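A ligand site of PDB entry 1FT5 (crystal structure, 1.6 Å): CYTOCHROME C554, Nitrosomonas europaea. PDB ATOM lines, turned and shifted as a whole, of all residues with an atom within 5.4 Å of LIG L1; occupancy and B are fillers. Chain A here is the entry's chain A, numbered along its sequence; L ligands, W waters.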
ATOM      1  N   GLY A   7       0.672 -27.108  14.073  1.00  0.00           N
ATOM      2  CA  GLY A   7       1.110 -25.746  14.335  1.00  0.00           C
ATOM      3  C   GLY A   7       0.022 -24.909  14.965  1.00  0.00           C
ATOM      4  O   GLY A   7      -1.119 -25.300  14.975  1.00  0.00           O
ATOM      5  N   LYS A  10      -3.962 -22.177  13.029  1.00  0.00           N
ATOM      6  CA  LYS A  10      -5.439 -22.222  13.006  1.00  0.00           C
ATOM      7  C   LYS A  10      -5.989 -22.104  14.415  1.00  0.00           C
ATOM      8  O   LYS A  10      -7.030 -21.456  14.627  1.00  0.00           O
ATOM      9  CB  LYS A  10      -5.955 -23.476  12.292  1.00  0.00           C
ATOM     10  CG  LYS A  10      -5.690 -23.429  10.741  1.00  0.00           C
ATOM     11  CD  LYS A  10      -5.507 -24.793  10.136  1.00  0.00           C
ATOM     12  CE  LYS A  10      -4.473 -24.730   8.979  1.00  0.00           C
ATOM     13  NZ  LYS A  10      -3.075 -24.961   9.505  1.00  0.00           N
ATOM     14  N   CYS A  11      -5.328 -22.700  15.406  1.00  0.00           N
ATOM     15  CA  CYS A  11      -5.862 -22.502  16.737  1.00  0.00           C
ATOM     16  C   CYS A  11      -5.929 -21.028  17.088  1.00  0.00           C
ATOM     17  O   CYS A  11      -6.900 -20.578  17.709  1.00  0.00           O
ATOM     18  CB  CYS A  11      -4.953 -23.164  17.810  1.00  0.00           C
ATOM     19  SG  CYS A  11      -4.280 -24.810  17.430  1.00  0.00           S
ATOM     20  N   SER A  13      -6.153 -18.440  15.228  1.00  0.00           N
ATOM     21  CA  SER A  13      -7.103 -17.634  14.450  1.00  0.00           C
ATOM     22  C   SER A  13      -8.513 -17.730  15.020  1.00  0.00           C
ATOM     23  O   SER A  13      -9.263 -16.730  14.956  1.00  0.00           O
ATOM     24  CB  SER A  13      -7.061 -18.044  12.976  1.00  0.00           C
ATOM     25  OG  SER A  13      -7.700 -19.276  12.799  1.00  0.00           O
ATOM     26  N   CYS A  14      -8.889 -18.869  15.577  1.00  0.00           N
ATOM     27  CA  CYS A  14     -10.208 -19.029  16.196  1.00  0.00           C
ATOM     28  C   CYS A  14     -10.218 -18.671  17.645  1.00  0.00           C
ATOM     29  O   CYS A  14     -11.301 -18.477  18.211  1.00  0.00           O
ATOM     30  CB  CYS A  14     -10.715 -20.439  16.102  1.00  0.00           C
ATOM     31  SG  CYS A  14     -11.250 -20.796  14.382  1.00  0.00           S
ATOM     32  N   HIS A  15      -9.028 -18.611  18.279  1.00  0.00           N
ATOM     33  CA  HIS A  15      -8.957 -18.361  19.697  1.00  0.00           C
ATOM     34  C   HIS A  15      -8.006 -17.239  19.931  1.00  0.00           C
ATOM     35  O   HIS A  15      -6.938 -17.402  20.571  1.00  0.00           O
ATOM     36  CB  HIS A  15      -8.467 -19.642  20.381  1.00  0.00           C
ATOM     37  CG  HIS A  15      -9.445 -20.767  20.260  1.00  0.00           C
ATOM     38  ND1 HIS A  15     -10.707 -20.735  20.824  1.00  0.00           N
ATOM     39  CD2 HIS A  15      -9.317 -22.013  19.708  1.00  0.00           C
ATOM     40  CE1 HIS A  15     -11.262 -21.940  20.632  1.00  0.00           C
ATOM     41  NE2 HIS A  15     -10.488 -22.797  19.935  1.00  0.00           N
ATOM     42  N   CYS A  88       0.209 -24.180  21.330  1.00  0.00           N
ATOM     43  CA  CYS A  88      -1.089 -24.737  21.712  1.00  0.00           C
ATOM     44  C   CYS A  88      -1.163 -26.235  21.807  1.00  0.00           C
ATOM     45  O   CYS A  88      -1.731 -26.814  22.693  1.00  0.00           O
ATOM     46  CB  CYS A  88      -2.143 -24.228  20.682  1.00  0.00           C
ATOM     47  SG  CYS A  88      -2.011 -22.519  20.210  1.00  0.00           S
ATOM     48  N   GLU A  89      -0.634 -26.924  20.775  1.00  0.00           N
ATOM     49  CA  GLU A  89      -0.742 -28.355  20.713  1.00  0.00           C
ATOM     50  C   GLU A  89       0.184 -29.047  21.736  1.00  0.00           C
ATOM     51  O   GLU A  89      -0.062 -30.188  22.046  1.00  0.00           O
ATOM     52  CB  GLU A  89      -0.361 -28.818  19.325  1.00  0.00           C
ATOM     53  CG  GLU A  89      -1.376 -28.389  18.220  1.00  0.00           C
ATOM     54  CD  GLU A  89      -0.773 -28.602  16.837  1.00  0.00           C
ATOM     55  OE1 GLU A  89       0.251 -28.003  16.532  1.00  0.00           O
ATOM     56  OE2 GLU A  89      -1.325 -29.431  16.075  1.00  0.00           O
ATOM     57  N   HIS A  92      -2.601 -28.966  24.472  1.00  0.00           N
ATOM     58  CA  HIS A  92      -3.898 -29.473  24.087  1.00  0.00           C
ATOM     59  C   HIS A  92      -3.895 -30.683  23.174  1.00  0.00           C
ATOM     60  O   HIS A  92      -4.955 -31.224  22.886  1.00  0.00           O
ATOM     61  CB  HIS A  92      -4.678 -28.326  23.405  1.00  0.00           C
ATOM     62  CG  HIS A  92      -4.986 -27.225  24.361  1.00  0.00           C
ATOM     63  ND1 HIS A  92      -5.945 -27.348  25.342  1.00  0.00           N
ATOM     64  CD2 HIS A  92      -4.452 -25.990  24.499  1.00  0.00           C
ATOM     65  CE1 HIS A  92      -5.948 -26.209  26.040  1.00  0.00           C
ATOM     66  NE2 HIS A  92      -5.071 -25.345  25.578  1.00  0.00           N
ATOM     67  N   GLY A  93      -2.710 -31.086  22.752  1.00  0.00           N
ATOM     68  CA  GLY A  93      -2.601 -32.277  21.878  1.00  0.00           C
ATOM     69  C   GLY A  93      -2.490 -31.865  20.435  1.00  0.00           C
ATOM     70  O   GLY A  93      -2.860 -30.775  20.036  1.00  0.00           O
ATOM     71  N   GLY A  95      -3.316 -31.282  16.805  1.00  0.00           N
ATOM     72  CA  GLY A  95      -4.636 -30.849  16.349  1.00  0.00           C
ATOM     73  C   GLY A  95      -5.072 -31.073  14.938  1.00  0.00           C
ATOM     74  O   GLY A  95      -6.198 -30.658  14.599  1.00  0.00           O
ATOM     75  N   PHE A  98      -8.570 -32.935  15.322  1.00  0.00           N
ATOM     76  CA  PHE A  98      -9.658 -32.348  16.082  1.00  0.00           C
ATOM     77  C   PHE A  98     -10.031 -30.952  15.718  1.00  0.00           C
ATOM     78  O   PHE A  98     -11.182 -30.543  15.992  1.00  0.00           O
ATOM     79  CB  PHE A  98      -9.433 -32.534  17.639  1.00  0.00           C
ATOM     80  CG  PHE A  98      -8.375 -31.620  18.294  1.00  0.00           C
ATOM     81  CD1 PHE A  98      -8.530 -30.231  18.345  1.00  0.00           C
ATOM     82  CD2 PHE A  98      -7.223 -32.176  18.947  1.00  0.00           C
ATOM     83  CE1 PHE A  98      -7.647 -29.386  19.004  1.00  0.00           C
ATOM     84  CE2 PHE A  98      -6.322 -31.313  19.621  1.00  0.00           C
ATOM     85  CZ  PHE A  98      -6.516 -29.949  19.658  1.00  0.00           C
ATOM     86  N   ARG A  99      -9.133 -30.194  15.088  1.00  0.00           N
ATOM     87  CA  ARG A  99      -9.395 -28.801  14.787  1.00  0.00           C
ATOM     88  C   ARG A  99     -10.602 -28.620  13.876  1.00  0.00           C
ATOM     89  O   ARG A  99     -11.338 -27.648  14.038  1.00  0.00           O
ATOM     90  CB  ARG A  99      -8.173 -28.137  14.207  1.00  0.00           C
ATOM     91  CG  ARG A  99      -7.840 -28.575  12.811  1.00  0.00           C
ATOM     92  CD  ARG A  99      -7.099 -27.440  12.120  1.00  0.00           C
ATOM     93  NE  ARG A  99      -6.307 -27.929  11.011  1.00  0.00           N
ATOM     94  CZ  ARG A  99      -6.773 -28.002   9.764  1.00  0.00           C
ATOM     95  NH1 ARG A  99      -8.025 -27.600   9.520  1.00  0.00           N
ATOM     96  NH2 ARG A  99      -6.013 -28.501   8.796  1.00  0.00           N
ATOM     97  N   HIS A 102     -13.684 -28.658  15.888  1.00  0.00           N
ATOM     98  CA  HIS A 102     -13.986 -27.374  16.592  1.00  0.00           C
ATOM     99  C   HIS A 102     -14.783 -26.480  15.634  1.00  0.00           C
ATOM    100  O   HIS A 102     -15.754 -25.831  16.051  1.00  0.00           O
ATOM    101  CB  HIS A 102     -12.732 -26.625  17.054  1.00  0.00           C
ATOM    102  CG  HIS A 102     -12.068 -27.323  18.196  1.00  0.00           C
ATOM    103  ND1 HIS A 102     -11.230 -26.658  19.100  1.00  0.00           N
ATOM    104  CD2 HIS A 102     -12.116 -28.644  18.495  1.00  0.00           C
ATOM    105  CE1 HIS A 102     -10.799 -27.645  19.911  1.00  0.00           C
ATOM    106  NE2 HIS A 102     -11.294 -28.831  19.600  1.00  0.00           N
ATOM    107  N   ARG A 103     -14.398 -26.464  14.347  1.00  0.00           N
ATOM    108  CA  ARG A 103     -15.100 -25.638  13.348  1.00  0.00           C
ATOM    109  C   ARG A 103     -16.514 -26.182  13.118  1.00  0.00           C
ATOM    110  O   ARG A 103     -17.525 -25.418  13.234  1.00  0.00           O
ATOM    111  CB  ARG A 103     -14.353 -25.668  11.997  1.00  0.00           C
ATOM    112  CG  ARG A 103     -15.016 -24.751  10.964  1.00  0.00           C
ATOM    113  CD  ARG A 103     -14.739 -25.136   9.484  1.00  0.00           C
ATOM    114  NE  ARG A 103     -15.979 -25.571   8.823  1.00  0.00           N
ATOM    115  CZ  ARG A 103     -16.496 -25.026   7.730  1.00  0.00           C
ATOM    116  NH1 ARG A 103     -15.885 -24.008   7.134  1.00  0.00           N
ATOM    117  NH2 ARG A 103     -17.650 -25.491   7.225  1.00  0.00           N
ATOM    118  N   GLY A 106     -18.701 -25.870  16.290  1.00  0.00           N
ATOM    119  CA  GLY A 106     -18.978 -24.458  16.543  1.00  0.00           C
ATOM    120  C   GLY A 106     -20.110 -23.999  15.612  1.00  0.00           C
ATOM    121  O   GLY A 106     -21.009 -23.286  16.038  1.00  0.00           O
ATOM    122  N   ARG A 118     -17.213 -34.055  24.434  1.00  0.00           N
ATOM    123  CA  ARG A 118     -15.742 -33.948  24.444  1.00  0.00           C
ATOM    124  C   ARG A 118     -15.150 -35.316  24.070  1.00  0.00           C
ATOM    125  O   ARG A 118     -14.030 -35.379  23.562  1.00  0.00           O
ATOM    126  CB  ARG A 118     -15.238 -33.574  25.850  1.00  0.00           C
ATOM    127  CG  ARG A 118     -15.381 -32.099  26.166  1.00  0.00           C
ATOM    128  CD  ARG A 118     -14.677 -31.787  27.506  1.00  0.00           C
ATOM    129  NE  ARG A 118     -14.841 -30.383  27.686  1.00  0.00           N
ATOM    130  CZ  ARG A 118     -15.866 -29.871  28.346  1.00  0.00           C
ATOM    131  NH1 ARG A 118     -16.764 -30.672  28.897  1.00  0.00           N
ATOM    132  NH2 ARG A 118     -16.066 -28.581  28.332  1.00  0.00           N
ATOM    133  N   LEU A 121     -13.853 -35.340  20.697  1.00  0.00           N
ATOM    134  CA  LEU A 121     -12.565 -34.649  20.538  1.00  0.00           C
ATOM    135  C   LEU A 121     -11.420 -35.481  21.103  1.00  0.00           C
ATOM    136  O   LEU A 121     -10.335 -35.497  20.506  1.00  0.00           O
ATOM    137  CB  LEU A 121     -12.567 -33.302  21.281  1.00  0.00           C
ATOM    138  CG  LEU A 121     -13.673 -32.332  20.828  1.00  0.00           C
ATOM    139  CD1 LEU A 121     -13.597 -31.152  21.745  1.00  0.00           C
ATOM    140  CD2 LEU A 121     -13.461 -31.893  19.395  1.00  0.00           C
ATOM    141  N   GLN A 126      -7.469 -34.862  21.191  1.00  0.00           N
ATOM    142  CA  GLN A 126      -7.360 -33.685  22.091  1.00  0.00           C
ATOM    143  C   GLN A 126      -7.127 -34.172  23.518  1.00  0.00           C
ATOM    144  O   GLN A 126      -7.673 -35.163  23.969  1.00  0.00           O
ATOM    145  CB  GLN A 126      -8.645 -32.805  21.977  1.00  0.00           C
ATOM    146  CG  GLN A 126      -8.489 -31.503  22.801  1.00  0.00           C
ATOM    147  CD  GLN A 126      -9.504 -30.449  22.440  1.00  0.00           C
ATOM    148  OE1 GLN A 126     -10.220 -30.614  21.409  1.00  0.00           O
ATOM    149  NE2 GLN A 126      -9.569 -29.390  23.187  1.00  0.00           N
ATOM    150  N   PHE A 128      -7.464 -33.513  27.516  1.00  0.00           N
ATOM    151  CA  PHE A 128      -8.206 -32.819  28.551  1.00  0.00           C
ATOM    152  C   PHE A 128      -7.663 -33.099  29.926  1.00  0.00           C
ATOM    153  O   PHE A 128      -8.341 -32.813  30.900  1.00  0.00           O
ATOM    154  CB  PHE A 128      -9.683 -33.251  28.493  1.00  0.00           C
ATOM    155  CG  PHE A 128     -10.314 -32.915  27.179  1.00  0.00           C
ATOM    156  CD1 PHE A 128     -10.840 -31.654  26.975  1.00  0.00           C
ATOM    157  CD2 PHE A 128     -10.370 -33.860  26.132  1.00  0.00           C
ATOM    158  CE1 PHE A 128     -11.415 -31.295  25.759  1.00  0.00           C
ATOM    159  CE2 PHE A 128     -10.962 -33.514  24.887  1.00  0.00           C
ATOM    160  CZ  PHE A 128     -11.486 -32.217  24.686  1.00  0.00           C
ATOM    161  N   LYS A 183     -14.133 -17.033  29.026  1.00  0.00           N
ATOM    162  CA  LYS A 183     -15.421 -17.741  29.114  1.00  0.00           C
ATOM    163  C   LYS A 183     -15.837 -18.458  27.833  1.00  0.00           C
ATOM    164  O   LYS A 183     -15.766 -17.850  26.760  1.00  0.00           O
ATOM    165  CB  LYS A 183     -16.493 -16.684  29.437  1.00  0.00           C
ATOM    166  CG  LYS A 183     -16.379 -16.181  30.845  1.00  0.00           C
ATOM    167  CD  LYS A 183     -16.996 -17.101  31.893  1.00  0.00           C
ATOM    168  CE  LYS A 183     -17.912 -18.154  31.267  1.00  0.00           C
ATOM    169  NZ  LYS A 183     -18.156 -19.292  32.211  1.00  0.00           N
ATOM    170  N   LEU A 184     -16.245 -19.724  27.983  1.00  0.00           N
ATOM    171  CA  LEU A 184     -16.713 -20.557  26.876  1.00  0.00           C
ATOM    172  C   LEU A 184     -18.249 -20.532  26.864  1.00  0.00           C
ATOM    173  O   LEU A 184     -18.889 -20.455  27.926  1.00  0.00           O
ATOM    174  CB  LEU A 184     -16.306 -21.997  27.084  1.00  0.00           C
ATOM    175  CG  LEU A 184     -14.755 -22.217  26.954  1.00  0.00           C
ATOM    176  CD1 LEU A 184     -14.404 -23.622  27.527  1.00  0.00           C
ATOM    177  CD2 LEU A 184     -14.317 -22.103  25.480  1.00  0.00           C
ATOM    178  N   GLU A 185     -18.834 -20.597  25.666  1.00  0.00           N
ATOM    179  CA  GLU A 185     -20.310 -20.690  25.556  1.00  0.00           C
ATOM    180  C   GLU A 185     -20.761 -22.097  25.942  1.00  0.00           C
ATOM    181  O   GLU A 185     -21.880 -22.303  26.439  1.00  0.00           O
ATOM    182  CB  GLU A 185     -20.732 -20.360  24.134  1.00  0.00           C
ATOM    183  CG  GLU A 185     -20.520 -18.923  23.791  1.00  0.00           C
ATOM    184  CD  GLU A 185     -21.366 -17.980  24.649  1.00  0.00           C
ATOM    185  OE1 GLU A 185     -22.380 -18.416  25.255  1.00  0.00           O
ATOM    186  OE2 GLU A 185     -21.025 -16.784  24.713  1.00  0.00           O
ATOM    187  N   GLY A 186     -19.921 -23.095  25.693  1.00  0.00           N
ATOM    188  CA  GLY A 186     -20.259 -24.444  26.084  1.00  0.00           C
ATOM    189  C   GLY A 186     -20.634 -25.377  24.942  1.00  0.00           C
ATOM    190  O   GLY A 186     -21.495 -26.245  25.108  1.00  0.00           O
ATOM    191  N   VAL A 187     -19.983 -25.197  23.807  1.00  0.00           N
ATOM    192  CA  VAL A 187     -20.217 -26.040  22.632  1.00  0.00           C
ATOM    193  C   VAL A 187     -19.923 -27.484  23.035  1.00  0.00           C
ATOM    194  O   VAL A 187     -20.661 -28.397  22.665  1.00  0.00           O
ATOM    195  CB  VAL A 187     -19.263 -25.636  21.492  1.00  0.00           C
ATOM    196  CG1 VAL A 187     -19.333 -26.656  20.324  1.00  0.00           C
ATOM    197  CG2 VAL A 187     -19.579 -24.225  21.024  1.00  0.00           C
ATOM    198  N   PHE A 188     -18.845 -27.751  23.781  1.00  0.00           N
ATOM    199  CA  PHE A 188     -18.542 -29.126  24.146  1.00  0.00           C
ATOM    200  C   PHE A 188     -18.993 -29.467  25.515  1.00  0.00           C
ATOM    201  O   PHE A 188     -18.984 -28.599  26.391  1.00  0.00           O
ATOM    202  CB  PHE A 188     -17.015 -29.351  23.981  1.00  0.00           C
ATOM    203  CG  PHE A 188     -16.543 -29.178  22.560  1.00  0.00           C
ATOM    204  CD1 PHE A 188     -15.908 -28.032  22.160  1.00  0.00           C
ATOM    205  CD2 PHE A 188     -16.876 -30.147  21.593  1.00  0.00           C
ATOM    206  CE1 PHE A 188     -15.577 -27.809  20.819  1.00  0.00           C
ATOM    207  CE2 PHE A 188     -16.554 -29.942  20.238  1.00  0.00           C
ATOM    208  CZ  PHE A 188     -15.922 -28.795  19.861  1.00  0.00           C
ATOM    209  N   HIS A 197     -11.598 -27.522  35.003  1.00  0.00           N
ATOM    210  CA  HIS A 197     -12.343 -26.748  34.005  1.00  0.00           C
ATOM    211  C   HIS A 197     -13.462 -25.826  34.594  1.00  0.00           C
ATOM    212  O   HIS A 197     -13.537 -24.652  34.270  1.00  0.00           O
ATOM    213  CB  HIS A 197     -13.007 -27.747  33.011  1.00  0.00           C
ATOM    214  CG  HIS A 197     -13.816 -27.071  31.943  1.00  0.00           C
ATOM    215  ND1 HIS A 197     -13.287 -26.659  30.742  1.00  0.00           N
ATOM    216  CD2 HIS A 197     -15.133 -26.720  31.904  1.00  0.00           C
ATOM    217  CE1 HIS A 197     -14.222 -26.085  30.004  1.00  0.00           C
ATOM    218  NE2 HIS A 197     -15.364 -26.117  30.690  1.00  0.00           N
HETATM  219  C1  LIG L   1     -13.113 -24.933  21.990  1.00  0.00           C
HETATM  220  C2  LIG L   1      -8.323 -25.553  21.641  1.00  0.00           C
HETATM  221  C3  LIG L   1      -8.635 -24.816  16.838  1.00  0.00           C
HETATM  222  C4  LIG L   1     -13.225 -23.204  17.452  1.00  0.00           C
HETATM  223  C5  LIG L   1     -11.786 -25.214  22.303  1.00  0.00           C
HETATM  224  C6  LIG L   1     -11.331 -25.626  23.625  1.00  0.00           C
HETATM  225  C7  LIG L   1      -9.961 -25.730  23.521  1.00  0.00           C
HETATM  226  C8  LIG L   1      -9.626 -25.458  22.164  1.00  0.00           C
HETATM  227  C9  LIG L   1      -8.942 -26.123  24.607  1.00  0.00           C
HETATM  228  C10 LIG L   1     -12.187 -25.884  24.823  1.00  0.00           C
HETATM  229  C11 LIG L   1     -12.748 -27.301  24.808  1.00  0.00           C
HETATM  230  C12 LIG L   1     -13.460 -27.706  26.085  1.00  0.00           C
HETATM  231  O1  LIG L   1     -14.635 -27.187  26.282  1.00  0.00           O
HETATM  232  O2  LIG L   1     -12.942 -28.517  26.901  1.00  0.00           O
HETATM  233  C13 LIG L   1      -8.025 -25.396  20.298  1.00  0.00           C
HETATM  234  C14 LIG L   1      -6.746 -25.669  19.757  1.00  0.00           C
HETATM  235  C15 LIG L   1      -6.830 -25.577  18.376  1.00  0.00           C
HETATM  236  C16 LIG L   1      -8.188 -25.181  18.097  1.00  0.00           C
HETATM  237  C17 LIG L   1      -5.479 -26.041  20.564  1.00  0.00           C
HETATM  238  C18 LIG L   1      -5.721 -25.814  17.317  1.00  0.00           C
HETATM  239  C19 LIG L   1      -5.359 -27.291  17.089  1.00  0.00           C
HETATM  240  C20 LIG L   1      -9.886 -24.260  16.623  1.00  0.00           C
HETATM  241  C21 LIG L   1     -10.289 -23.688  15.333  1.00  0.00           C
HETATM  242  C22 LIG L   1     -11.539 -23.156  15.558  1.00  0.00           C
HETATM  243  C23 LIG L   1     -11.930 -23.461  16.880  1.00  0.00           C
HETATM  244  C24 LIG L   1      -9.455 -23.644  14.033  1.00  0.00           C
HETATM  245  C25 LIG L   1     -12.344 -22.293  14.582  1.00  0.00           C
HETATM  246  C26 LIG L   1     -12.804 -22.831  13.241  1.00  0.00           C
HETATM  247  C27 LIG L   1     -13.594 -23.615  18.732  1.00  0.00           C
HETATM  248  C28 LIG L   1     -14.889 -23.489  19.273  1.00  0.00           C
HETATM  249  C29 LIG L   1     -14.871 -24.005  20.514  1.00  0.00           C
HETATM  250  C30 LIG L   1     -13.530 -24.465  20.757  1.00  0.00           C
HETATM  251  C31 LIG L   1     -16.111 -22.850  18.506  1.00  0.00           C
HETATM  252  C32 LIG L   1     -16.003 -23.914  21.490  1.00  0.00           C
HETATM  253  C33 LIG L   1     -16.061 -22.617  22.254  1.00  0.00           C
HETATM  254  C34 LIG L   1     -17.142 -22.440  23.315  1.00  0.00           C
HETATM  255  O3  LIG L   1     -17.452 -21.239  23.532  1.00  0.00           O
HETATM  256  O4  LIG L   1     -17.598 -23.408  23.915  1.00  0.00           O
HETATM  257  N1  LIG L   1     -10.730 -25.115  21.407  1.00  0.00           N
HETATM  258  N2  LIG L   1      -8.938 -25.076  19.290  1.00  0.00           N
HETATM  259  N3  LIG L   1     -10.891 -24.113  17.584  1.00  0.00           N
HETATM  260  N4  LIG L   1     -12.774 -24.248  19.672  1.00  0.00           N
HETATM  261 FE1  LIG L   1     -10.866 -24.648  19.484  1.00  0.00          FE
HETATM  262  C1  LG2 L   2      -7.732 -23.855  28.068  1.00  0.00           C
HETATM  263  C2  LG2 L   2      -6.701 -22.244  23.576  1.00  0.00           C
HETATM  264  C3  LG2 L   2      -1.943 -22.837  24.549  1.00  0.00           C
HETATM  265  C4  LG2 L   2      -3.080 -25.020  28.725  1.00  0.00           C
HETATM  266  C5  LG2 L   2      -7.833 -23.332  26.777  1.00  0.00           C
HETATM  267  C6  LG2 L   2      -9.068 -22.955  26.156  1.00  0.00           C
HETATM  268  C7  LG2 L   2      -8.795 -22.538  24.906  1.00  0.00           C
HETATM  269  C8  LG2 L   2      -7.382 -22.620  24.725  1.00  0.00           C
HETATM  270  C9  LG2 L   2      -9.781 -22.052  23.829  1.00  0.00           C
HETATM  271  C10 LG2 L   2     -10.491 -23.047  26.814  1.00  0.00           C
HETATM  272  C11 LG2 L   2     -10.953 -21.620  27.346  1.00  0.00           C
HETATM  273  C12 LG2 L   2      -9.922 -20.962  28.304  1.00  0.00           C
HETATM  274  O1  LG2 L   2      -9.605 -21.573  29.292  1.00  0.00           O
HETATM  275  O2  LG2 L   2      -9.464 -19.862  27.988  1.00  0.00           O
HETATM  276  C13 LG2 L   2      -5.284 -22.288  23.444  1.00  0.00           C
HETATM  277  C14 LG2 L   2      -4.586 -21.806  22.284  1.00  0.00           C
HETATM  278  C15 LG2 L   2      -3.236 -21.929  22.557  1.00  0.00           C
HETATM  279  C16 LG2 L   2      -3.175 -22.488  23.898  1.00  0.00           C
HETATM  280  C17 LG2 L   2      -5.258 -21.266  21.022  1.00  0.00           C
HETATM  281  C18 LG2 L   2      -2.023 -21.578  21.759  1.00  0.00           C
HETATM  282  C19 LG2 L   2      -1.962 -20.071  21.426  1.00  0.00           C
HETATM  283  C20 LG2 L   2      -1.887 -23.495  25.770  1.00  0.00           C
HETATM  284  C21 LG2 L   2      -0.666 -23.963  26.326  1.00  0.00           C
HETATM  285  C22 LG2 L   2      -0.966 -24.618  27.429  1.00  0.00           C
HETATM  286  C23 LG2 L   2      -2.384 -24.531  27.641  1.00  0.00           C
HETATM  287  C24 LG2 L   2       0.743 -23.757  25.728  1.00  0.00           C
HETATM  288  C25 LG2 L   2       0.025 -25.389  28.343  1.00  0.00           C
HETATM  289  C26 LG2 L   2       1.273 -24.684  28.830  1.00  0.00           C
HETATM  290  C27 LG2 L   2      -4.464 -24.867  28.938  1.00  0.00           C
HETATM  291  C28 LG2 L   2      -5.163 -25.357  30.103  1.00  0.00           C
HETATM  292  C29 LG2 L   2      -6.486 -24.972  29.917  1.00  0.00           C
HETATM  293  C30 LG2 L   2      -6.534 -24.294  28.650  1.00  0.00           C
HETATM  294  C31 LG2 L   2      -4.581 -26.182  31.224  1.00  0.00           C
HETATM  295  C32 LG2 L   2      -7.679 -25.349  30.778  1.00  0.00           C
HETATM  296  C33 LG2 L   2      -8.473 -26.449  30.136  1.00  0.00           C
HETATM  297  C34 LG2 L   2      -9.952 -26.534  30.564  1.00  0.00           C
HETATM  298  O3  LG2 L   2     -10.628 -27.399  30.001  1.00  0.00           O
HETATM  299  O4  LG2 L   2     -10.360 -25.746  31.428  1.00  0.00           O
HETATM  300  N1  LG2 L   2      -6.804 -23.111  25.889  1.00  0.00           N
HETATM  301  N2  LG2 L   2      -4.416 -22.727  24.455  1.00  0.00           N
HETATM  302  N3  LG2 L   2      -2.938 -23.831  26.571  1.00  0.00           N
HETATM  303  N4  LG2 L   2      -5.297 -24.197  28.021  1.00  0.00           N
HETATM  304 FE1  LG2 L   2      -4.867 -23.432  26.249  1.00  0.00          FE
HETATM  305  O   HOH W   1     -16.694 -25.907  24.879  1.00  0.00           O
HETATM  306  O   HOH W   2      -8.092 -29.167  25.779  1.00  0.00           O
HETATM  307  O   HOH W   3     -10.137 -28.117  27.271  1.00  0.00           O
HETATM  308  O   HOH W   4     -11.965 -29.780  29.847  1.00  0.00           O
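Lys 10 touches LIG L1. Cys 88 touches LIG L1 (CB to C17, 3.8 Å). ND1 of His 92 touches C9 of LIG L1 (3.3 Å). Gly 95 touches LIG L1 (CA to C19, 3.7 Å). Phe 98 touches LIG L1. Arg 103 touches LIG L1 (CB to C26, 3.5 Å). Gly 106 touches LIG L1 (CA to C31, 3.8 Å). NE2 of Gln 126 touches C9 of LIG L1 (3.6 Å). CE1 of Phe 128 touches O2 of LIG L1 (3.4 Å). Leu 184 touches LIG L1 (CA to O3, 3.5 Å). Phe 188 touches LIG L1 (CE1 to C29, 3.9 Å). CE1 of His 197 touches O1 of LIG L1, 3.9 Å away. Hydrophobic or aromatic side chains within 4 Å of LIG L1: His 15, His 92, Phe 98, His 102, Phe 128, Leu 184, Val 187, Phe 188 and His 197. Of the 27 residues printed, 20 come within 4 Å of LIG L1.
Water W1 lies within hydrogen-bond range of an oxygen (O1) of LIG L1 and the backbone NH (N) of Phe 188. Water W3 lies within hydrogen-bond range of an oxygen (O2) of LIG L1 and an oxygen (O3) of LG2 L2. Water W4 lies within hydrogen-bond range of an oxygen (O3) of LG2 L2 (2.7 Å) and an oxygen (O2) of LIG L1 (3.4 Å). Water W2 lies within hydrogen-bond range of a ring nitrogen (ND1) of His 92 (2.8 Å) and the side-chain amide nitrogen of Gln 126 (3.0 Å).
A carbon (C18) of LIG L1 is bonded to the side-chain sulfur (SG) of Cys 11 (1.8 Å). A carbon (C25) of LIG L1 is covalently linked to the side-chain sulfur (SG) of Cys 14, at 1.9 Å. An iron atom (FE1) of LIG L1 is bound by a ring nitrogen (NE2) of His 15 (1.9 Å). An iron atom (FE1) of LIG L1 is bound by a ring nitrogen (ND1) of His 102, at 2.1 Å. N of Glu 185 lies within hydrogen-bond range of O3 of LIG L1, at 2.6 Å. O2 of LIG L1 is in salt-bridge range of NE of Arg 118 (2.8 Å). The backbone NH (N) of Gly 186 sits at hydrogen-bond distance from an oxygen (O4) of LIG L1, 2.9 Å away. O4 of LIG L1 lies within hydrogen-bond range of N of Val 187, at 3.0 Å. An iron atom (FE1) of LG2 L2 is bound by a ring nitrogen (NE2) of His 92 (2.0 Å). The side-chain sulfur (SG) of Cys 88 is bonded to a carbon (C18) of LG2 L2 (1.8 Å). ND1 of His 197 sits at hydrogen-bond distance from O3 of LG2 L2 (2.9 Å).
NE2 of His 102 sits at hydrogen-bond distance from OE1 of Gln 126 (2.8 Å). NH2 of Arg 118 sits at hydrogen-bond distance from NE2 of His 197 (3.5 Å). OG of Ser 13 lies within hydrogen-bond range of O of Lys 10, at 2.9 Å. The backbone NH (N) of Gln 126 sits at hydrogen-bond distance from the backbone carbonyl oxygen (O) of Leu 121, at 3.0 Å. N of Gly 95 lies within hydrogen-bond range of OE2 of Glu 89, 2.8 Å away.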
